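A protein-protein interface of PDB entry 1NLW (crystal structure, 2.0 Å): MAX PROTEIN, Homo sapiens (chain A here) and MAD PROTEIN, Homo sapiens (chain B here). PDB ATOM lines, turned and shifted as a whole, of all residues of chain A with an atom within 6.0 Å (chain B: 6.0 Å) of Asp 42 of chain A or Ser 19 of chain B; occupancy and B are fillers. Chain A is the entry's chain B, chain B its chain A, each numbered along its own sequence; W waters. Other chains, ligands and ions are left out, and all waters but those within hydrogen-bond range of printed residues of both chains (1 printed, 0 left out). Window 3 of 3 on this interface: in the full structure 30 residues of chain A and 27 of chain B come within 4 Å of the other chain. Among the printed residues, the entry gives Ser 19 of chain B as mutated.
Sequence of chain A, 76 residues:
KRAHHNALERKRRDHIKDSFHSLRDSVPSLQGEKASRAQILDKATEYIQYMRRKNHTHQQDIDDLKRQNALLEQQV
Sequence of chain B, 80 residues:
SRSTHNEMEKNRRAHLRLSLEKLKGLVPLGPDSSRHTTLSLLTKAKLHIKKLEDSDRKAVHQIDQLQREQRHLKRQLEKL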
ATOM      1  N   ARG A  37      23.692 -21.492  10.334  1.00  0.00           N
ATOM      2  CA  ARG A  37      24.464 -20.752  11.325  1.00  0.00           C
ATOM      3  C   ARG A  37      24.523 -19.268  10.955  1.00  0.00           C
ATOM      4  O   ARG A  37      24.529 -18.414  11.824  1.00  0.00           O
ATOM      5  CB  ARG A  37      25.878 -21.326  11.449  1.00  0.00           C
ATOM      6  CG  ARG A  37      25.907 -22.736  12.014  1.00  0.00           C
ATOM      7  CD  ARG A  37      27.323 -23.250  12.253  1.00  0.00           C
ATOM      8  NE  ARG A  37      27.301 -24.531  12.960  1.00  0.00           N
ATOM      9  CZ  ARG A  37      28.338 -25.069  13.604  1.00  0.00           C
ATOM     10  NH1 ARG A  37      29.515 -24.452  13.649  1.00  0.00           N
ATOM     11  NH2 ARG A  37      28.191 -26.236  14.212  1.00  0.00           N
ATOM     12  N   ALA A  38      24.551 -18.967   9.659  1.00  0.00           N
ATOM     13  CA  ALA A  38      24.590 -17.573   9.225  1.00  0.00           C
ATOM     14  C   ALA A  38      23.293 -16.871   9.652  1.00  0.00           C
ATOM     15  O   ALA A  38      23.326 -15.782  10.222  1.00  0.00           O
ATOM     16  CB  ALA A  38      24.768 -17.493   7.687  1.00  0.00           C
ATOM     17  N   GLN A  39      22.150 -17.501   9.398  1.00  0.00           N
ATOM     18  CA  GLN A  39      20.860 -16.914   9.769  1.00  0.00           C
ATOM     19  C   GLN A  39      20.713 -16.697  11.280  1.00  0.00           C
ATOM     20  O   GLN A  39      20.132 -15.696  11.729  1.00  0.00           O
ATOM     21  CB  GLN A  39      19.718 -17.805   9.263  1.00  0.00           C
ATOM     22  CG  GLN A  39      19.372 -17.586   7.782  1.00  0.00           C
ATOM     23  CD  GLN A  39      18.512 -18.696   7.209  1.00  0.00           C
ATOM     24  OE1 GLN A  39      17.987 -18.582   6.093  1.00  0.00           O
ATOM     25  NE2 GLN A  39      18.370 -19.780   7.958  1.00  0.00           N
ATOM     26  N   ILE A  40      21.240 -17.630  12.067  1.00  0.00           N
ATOM     27  CA  ILE A  40      21.157 -17.512  13.518  1.00  0.00           C
ATOM     28  C   ILE A  40      21.935 -16.286  14.011  1.00  0.00           C
ATOM     29  O   ILE A  40      21.442 -15.516  14.828  1.00  0.00           O
ATOM     30  CB  ILE A  40      21.703 -18.800  14.214  1.00  0.00           C
ATOM     31  CG1 ILE A  40      20.775 -19.989  13.900  1.00  0.00           C
ATOM     32  CG2 ILE A  40      21.816 -18.563  15.721  1.00  0.00           C
ATOM     33  CD1 ILE A  40      21.303 -21.351  14.352  1.00  0.00           C
ATOM     34  N   LEU A  41      23.163 -16.110  13.533  1.00  0.00           N
ATOM     35  CA  LEU A  41      23.950 -14.957  13.957  1.00  0.00           C
ATOM     36  C   LEU A  41      23.303 -13.639  13.556  1.00  0.00           C
ATOM     37  O   LEU A  41      23.212 -12.728  14.371  1.00  0.00           O
ATOM     38  CB  LEU A  41      25.361 -15.019  13.384  1.00  0.00           C
ATOM     39  CG  LEU A  41      26.164 -16.242  13.835  1.00  0.00           C
ATOM     40  CD1 LEU A  41      27.580 -16.138  13.290  1.00  0.00           C
ATOM     41  CD2 LEU A  41      26.160 -16.323  15.358  1.00  0.00           C
ATOM     42  N   ASP A  42      22.871 -13.544  12.304  1.00  0.00           N
ATOM     43  CA  ASP A  42      22.237 -12.326  11.783  1.00  0.00           C
ATOM     44  C   ASP A  42      20.910 -11.970  12.490  1.00  0.00           C
ATOM     45  O   ASP A  42      20.712 -10.833  12.893  1.00  0.00           O
ATOM     46  CB  ASP A  42      22.019 -12.482  10.271  1.00  0.00           C
ATOM     47  CG  ASP A  42      23.331 -12.464   9.475  1.00  0.00           C
ATOM     48  OD1 ASP A  42      23.314 -12.899   8.298  1.00  0.00           O
ATOM     49  OD2 ASP A  42      24.371 -12.005  10.012  1.00  0.00           O
ATOM     50  N   LYS A  43      20.009 -12.933  12.656  1.00  0.00           N
ATOM     51  CA  LYS A  43      18.745 -12.654  13.336  1.00  0.00           C
ATOM     52  C   LYS A  43      18.917 -12.357  14.825  1.00  0.00           C
ATOM     53  O   LYS A  43      18.199 -11.512  15.383  1.00  0.00           O
ATOM     54  CB  LYS A  43      17.757 -13.809  13.128  1.00  0.00           C
ATOM     55  CG  LYS A  43      16.933 -13.666  11.851  1.00  0.00           C
ATOM     56  CD  LYS A  43      17.826 -13.376  10.665  1.00  0.00           C
ATOM     57  CE  LYS A  43      17.146 -12.450   9.670  1.00  0.00           C
ATOM     58  NZ  LYS A  43      15.910 -13.042   9.101  1.00  0.00           N
ATOM     59  N   ALA A  44      19.866 -13.027  15.477  1.00  0.00           N
ATOM     60  CA  ALA A  44      20.099 -12.763  16.902  1.00  0.00           C
ATOM     61  C   ALA A  44      20.595 -11.328  17.023  1.00  0.00           C
ATOM     62  O   ALA A  44      20.190 -10.593  17.907  1.00  0.00           O
ATOM     63  CB  ALA A  44      21.158 -13.738  17.477  1.00  0.00           C
ATOM     64  N   THR A  45      21.501 -10.941  16.131  1.00  0.00           N
ATOM     65  CA  THR A  45      22.025  -9.581  16.132  1.00  0.00           C
ATOM     66  C   THR A  45      20.853  -8.616  16.001  1.00  0.00           C
ATOM     67  O   THR A  45      20.753  -7.658  16.742  1.00  0.00           O
ATOM     68  CB  THR A  45      22.974  -9.360  14.939  1.00  0.00           C
ATOM     69  OG1 THR A  45      24.124 -10.196  15.094  1.00  0.00           O
ATOM     70  CG2 THR A  45      23.392  -7.891  14.838  1.00  0.00           C
ATOM     71  N   GLU A  46      19.974  -8.882  15.043  1.00  0.00           N
ATOM     72  CA  GLU A  46      18.809  -8.033  14.821  1.00  0.00           C
ATOM     73  C   GLU A  46      17.928  -7.946  16.063  1.00  0.00           C
ATOM     74  O   GLU A  46      17.573  -6.856  16.515  1.00  0.00           O
ATOM     75  CB  GLU A  46      17.977  -8.567  13.652  1.00  0.00           C
ATOM     76  CG  GLU A  46      16.626  -7.865  13.488  1.00  0.00           C
ATOM     77  CD  GLU A  46      15.432  -8.760  13.829  1.00  0.00           C
ATOM     78  OE1 GLU A  46      15.129  -9.686  13.034  1.00  0.00           O
ATOM     79  OE2 GLU A  46      14.796  -8.538  14.890  1.00  0.00           O
ATOM     80  N   TYR A  47      17.567  -9.106  16.603  1.00  0.00           N
ATOM     81  CA  TYR A  47      16.729  -9.177  17.795  1.00  0.00           C
ATOM     82  C   TYR A  47      17.324  -8.393  18.973  1.00  0.00           C
ATOM     83  O   TYR A  47      16.603  -7.682  19.673  1.00  0.00           O
ATOM     84  CB  TYR A  47      16.509 -10.652  18.172  1.00  0.00           C
ATOM     85  CG  TYR A  47      15.461 -10.857  19.238  1.00  0.00           C
ATOM     86  CD1 TYR A  47      14.182 -10.314  19.091  1.00  0.00           C
ATOM     87  CD2 TYR A  47      15.745 -11.580  20.402  1.00  0.00           C
ATOM     88  CE1 TYR A  47      13.216 -10.476  20.065  1.00  0.00           C
ATOM     89  CE2 TYR A  47      14.779 -11.747  21.393  1.00  0.00           C
ATOM     90  CZ  TYR A  47      13.524 -11.190  21.216  1.00  0.00           C
ATOM     91  OH  TYR A  47      12.582 -11.304  22.193  1.00  0.00           O
ATOM     92  N   ALA B  14      34.489 -17.002   5.761  1.00  0.00           N
ATOM     93  CA  ALA B  14      34.797 -15.586   5.966  1.00  0.00           C
ATOM     94  C   ALA B  14      33.530 -14.787   6.288  1.00  0.00           C
ATOM     95  O   ALA B  14      33.508 -14.000   7.238  1.00  0.00           O
ATOM     96  CB  ALA B  14      35.484 -15.013   4.731  1.00  0.00           C
ATOM     97  N   HIS B  15      32.484 -14.981   5.491  1.00  0.00           N
ATOM     98  CA  HIS B  15      31.211 -14.296   5.714  1.00  0.00           C
ATOM     99  C   HIS B  15      30.626 -14.656   7.078  1.00  0.00           C
ATOM    100  O   HIS B  15      30.026 -13.818   7.746  1.00  0.00           O
ATOM    101  CB  HIS B  15      30.210 -14.666   4.623  1.00  0.00           C
ATOM    102  CG  HIS B  15      30.406 -13.905   3.350  1.00  0.00           C
ATOM    103  ND1 HIS B  15      30.007 -12.595   3.201  1.00  0.00           N
ATOM    104  CD2 HIS B  15      30.995 -14.257   2.184  1.00  0.00           C
ATOM    105  CE1 HIS B  15      30.342 -12.171   1.997  1.00  0.00           C
ATOM    106  NE2 HIS B  15      30.943 -13.159   1.360  1.00  0.00           N
ATOM    107  N   LEU B  16      30.810 -15.907   7.489  1.00  0.00           N
ATOM    108  CA  LEU B  16      30.298 -16.351   8.784  1.00  0.00           C
ATOM    109  C   LEU B  16      31.107 -15.647   9.862  1.00  0.00           C
ATOM    110  O   LEU B  16      30.585 -15.287  10.918  1.00  0.00           O
ATOM    111  CB  LEU B  16      30.432 -17.878   8.912  1.00  0.00           C
ATOM    112  CG  LEU B  16      29.859 -18.546  10.166  1.00  0.00           C
ATOM    113  CD1 LEU B  16      28.387 -18.172  10.329  1.00  0.00           C
ATOM    114  CD2 LEU B  16      30.009 -20.072  10.055  1.00  0.00           C
ATOM    115  N   ARG B  17      32.390 -15.438   9.582  1.00  0.00           N
ATOM    116  CA  ARG B  17      33.273 -14.763  10.521  1.00  0.00           C
ATOM    117  C   ARG B  17      32.829 -13.310  10.692  1.00  0.00           C
ATOM    118  O   ARG B  17      32.883 -12.765  11.792  1.00  0.00           O
ATOM    119  CB  ARG B  17      34.719 -14.817  10.016  1.00  0.00           C
ATOM    120  CG  ARG B  17      35.776 -14.753  11.116  1.00  0.00           C
ATOM    121  CD  ARG B  17      37.179 -15.029  10.549  1.00  0.00           C
ATOM    122  NE  ARG B  17      37.140 -16.062   9.516  1.00  0.00           N
ATOM    123  CZ  ARG B  17      38.209 -16.677   9.010  1.00  0.00           C
ATOM    124  NH1 ARG B  17      39.433 -16.376   9.441  1.00  0.00           N
ATOM    125  NH2 ARG B  17      38.048 -17.590   8.062  1.00  0.00           N
ATOM    126  N   LEU B  18      32.382 -12.687   9.603  1.00  0.00           N
ATOM    127  CA  LEU B  18      31.916 -11.303   9.652  1.00  0.00           C
ATOM    128  C   LEU B  18      30.658 -11.212  10.521  1.00  0.00           C
ATOM    129  O   LEU B  18      30.488 -10.270  11.282  1.00  0.00           O
ATOM    130  CB  LEU B  18      31.614 -10.779   8.238  1.00  0.00           C
ATOM    131  CG  LEU B  18      32.807 -10.474   7.312  1.00  0.00           C
ATOM    132  CD1 LEU B  18      32.309 -10.036   5.935  1.00  0.00           C
ATOM    133  CD2 LEU B  18      33.657  -9.371   7.926  1.00  0.00           C
ATOM    134  N   SER B  19      29.783 -12.201  10.424  1.00  0.00           N
ATOM    135  CA  SER B  19      28.570 -12.189  11.236  1.00  0.00           C
ATOM    136  C   SER B  19      28.915 -12.356  12.713  1.00  0.00           C
ATOM    137  O   SER B  19      28.325 -11.708  13.575  1.00  0.00           O
ATOM    138  CB  SER B  19      27.627 -13.286  10.770  1.00  0.00           C
ATOM    139  OG  SER B  19      27.223 -13.026   9.439  1.00  0.00           O
ATOM    140  N   LEU B  20      29.904 -13.195  13.000  1.00  0.00           N
ATOM    141  CA  LEU B  20      30.340 -13.420  14.380  1.00  0.00           C
ATOM    142  C   LEU B  20      30.965 -12.164  15.016  1.00  0.00           C
ATOM    143  O   LEU B  20      30.642 -11.796  16.154  1.00  0.00           O
ATOM    144  CB  LEU B  20      31.346 -14.573  14.413  1.00  0.00           C
ATOM    145  CG  LEU B  20      31.442 -15.343  15.731  1.00  0.00           C
ATOM    146  CD1 LEU B  20      30.148 -16.134  15.936  1.00  0.00           C
ATOM    147  CD2 LEU B  20      32.649 -16.284  15.689  1.00  0.00           C
ATOM    148  N   GLU B  21      31.864 -11.505  14.288  1.00  0.00           N
ATOM    149  CA  GLU B  21      32.504 -10.296  14.802  1.00  0.00           C
ATOM    150  C   GLU B  21      31.458  -9.223  15.117  1.00  0.00           C
ATOM    151  O   GLU B  21      31.550  -8.544  16.140  1.00  0.00           O
ATOM    152  CB  GLU B  21      33.512  -9.735  13.790  1.00  0.00           C
ATOM    153  CG  GLU B  21      34.799 -10.534  13.611  1.00  0.00           C
ATOM    154  CD  GLU B  21      35.658 -10.589  14.871  1.00  0.00           C
ATOM    155  OE1 GLU B  21      35.605  -9.647  15.686  1.00  0.00           O
ATOM    156  OE2 GLU B  21      36.406 -11.572  15.040  1.00  0.00           O
ATOM    157  N   LYS B  22      30.469  -9.070  14.240  1.00  0.00           N
ATOM    158  CA  LYS B  22      29.419  -8.077  14.457  1.00  0.00           C
ATOM    159  C   LYS B  22      28.692  -8.358  15.785  1.00  0.00           C
ATOM    160  O   LYS B  22      28.563  -7.471  16.629  1.00  0.00           O
ATOM    161  CB  LYS B  22      28.427  -8.084  13.286  1.00  0.00           C
ATOM    162  CG  LYS B  22      27.480  -6.892  13.277  1.00  0.00           C
ATOM    163  CD  LYS B  22      26.596  -6.858  12.024  1.00  0.00           C
ATOM    164  CE  LYS B  22      25.575  -7.995  12.021  1.00  0.00           C
ATOM    165  NZ  LYS B  22      24.642  -7.961  10.851  1.00  0.00           N
ATOM    166  N   LEU B  23      28.239  -9.596  15.977  1.00  0.00           N
ATOM    167  CA  LEU B  23      27.553  -9.983  17.215  1.00  0.00           C
ATOM    168  C   LEU B  23      28.493  -9.734  18.398  1.00  0.00           C
ATOM    169  O   LEU B  23      28.064  -9.355  19.487  1.00  0.00           O
ATOM    170  CB  LEU B  23      27.158 -11.469  17.157  1.00  0.00           C
ATOM    171  CG  LEU B  23      26.380 -12.045  18.346  1.00  0.00           C
ATOM    172  CD1 LEU B  23      25.153 -11.171  18.654  1.00  0.00           C
ATOM    173  CD2 LEU B  23      25.941 -13.473  18.022  1.00  0.00           C
ATOM    174  N   LYS B  24      29.782  -9.950  18.172  1.00  0.00           N
ATOM    175  CA  LYS B  24      30.782  -9.731  19.201  1.00  0.00           C
ATOM    176  C   LYS B  24      30.805  -8.248  19.563  1.00  0.00           C
ATOM    177  O   LYS B  24      31.032  -7.882  20.717  1.00  0.00           O
ATOM    178  CB  LYS B  24      32.161 -10.174  18.699  1.00  0.00           C
ATOM    179  CG  LYS B  24      33.311  -9.795  19.630  1.00  0.00           C
ATOM    180  CD  LYS B  24      34.647 -10.345  19.154  1.00  0.00           C
ATOM    181  CE  LYS B  24      34.770 -11.830  19.466  1.00  0.00           C
ATOM    182  NZ  LYS B  24      33.620 -12.631  18.940  1.00  0.00           N
HETATM  183  O   HOH W   1      25.998 -10.737  12.962  1.00  0.00           O
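Asp 42 of chain A touches just one residue of chain B: Ser 19. Ser 19 of chain B touches two residues of chain A. Of the printed residues of chain B, Ala 38 of chain A touches Leu 16 (3.97 Å). Printed residues of chain A within 4 Å of Leu 20 of chain B: Leu 41. Of the printed residues of chain A, Leu 23 of chain B touches Leu 41 and Thr 45. Of the printed residues of chain A, Leu 16 of chain B touches Ala 38 (3.97 Å) and Leu 41 (3.7 Å). Arg 17 of chain B touches none of the printed residues of chain A. Glu 21 of chain B touches none of the printed residues of chain A. The nearest printed residue of chain A that does not touch Leu 20 of chain B is Asp 42 of chain A (6.4 Å).
Water W1 lies within hydrogen-bond range of the backbone carbonyl oxygen (O) of Ser 19 of chain B (2.6 Å) and the side-chain hydroxyl (OG1) of Thr 45 of chain A (2.9 Å).
Hydrophobic or aromatic side chains of chain B within 4 Å of the printed part of chain A: Leu 16, Leu 20 and Leu 23. Printed residues of chain A that touch a printed residue of chain B: Ala 38, Leu 41, Asp 42 and Thr 45. Hydrophobic or aromatic side chains of chain A within 4 Å of the printed part of chain B: Leu 41. Among the printed residues, 8 pairs touch across the chains. Among the printed residues, no Asp or Glu carboxylate lies within 4 Å of a Lys or Arg side-chain nitrogen of the other chain.
The side-chain carboxylate of Asp 42 of chain A is in hydrogen-bond range of the side-chain hydroxyl of Ser 19 of chain B, 3.1 Å away.
The side-chain hydroxyl (OG1) of Thr 45 of chain A sits at hydrogen-bond distance from the backbone carbonyl oxygen (O) of Leu 41 of chain A (2.8 Å). The backbone carbonyl oxygen (O) of His 15 of chain B lies within hydrogen-bond range of the side-chain hydroxyl (OG) of Ser 19 of chain B, at 3.4 Å.
Among the printed residues, pairs that only touch across the chains: Thr 45 of chain A with Lys 22 of chain B, Leu 41 of chain A with Leu 16 of chain B, Leu 41 of chain A with Leu 20 of chain B, Leu 41 of chain A with Ser 19 of chain B, Thr 45 of chain A with Leu 23 of chain B, Leu 41 of chain A with Leu 23 of chain B and Ala 38 of chain A with Leu 16 of chain B.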
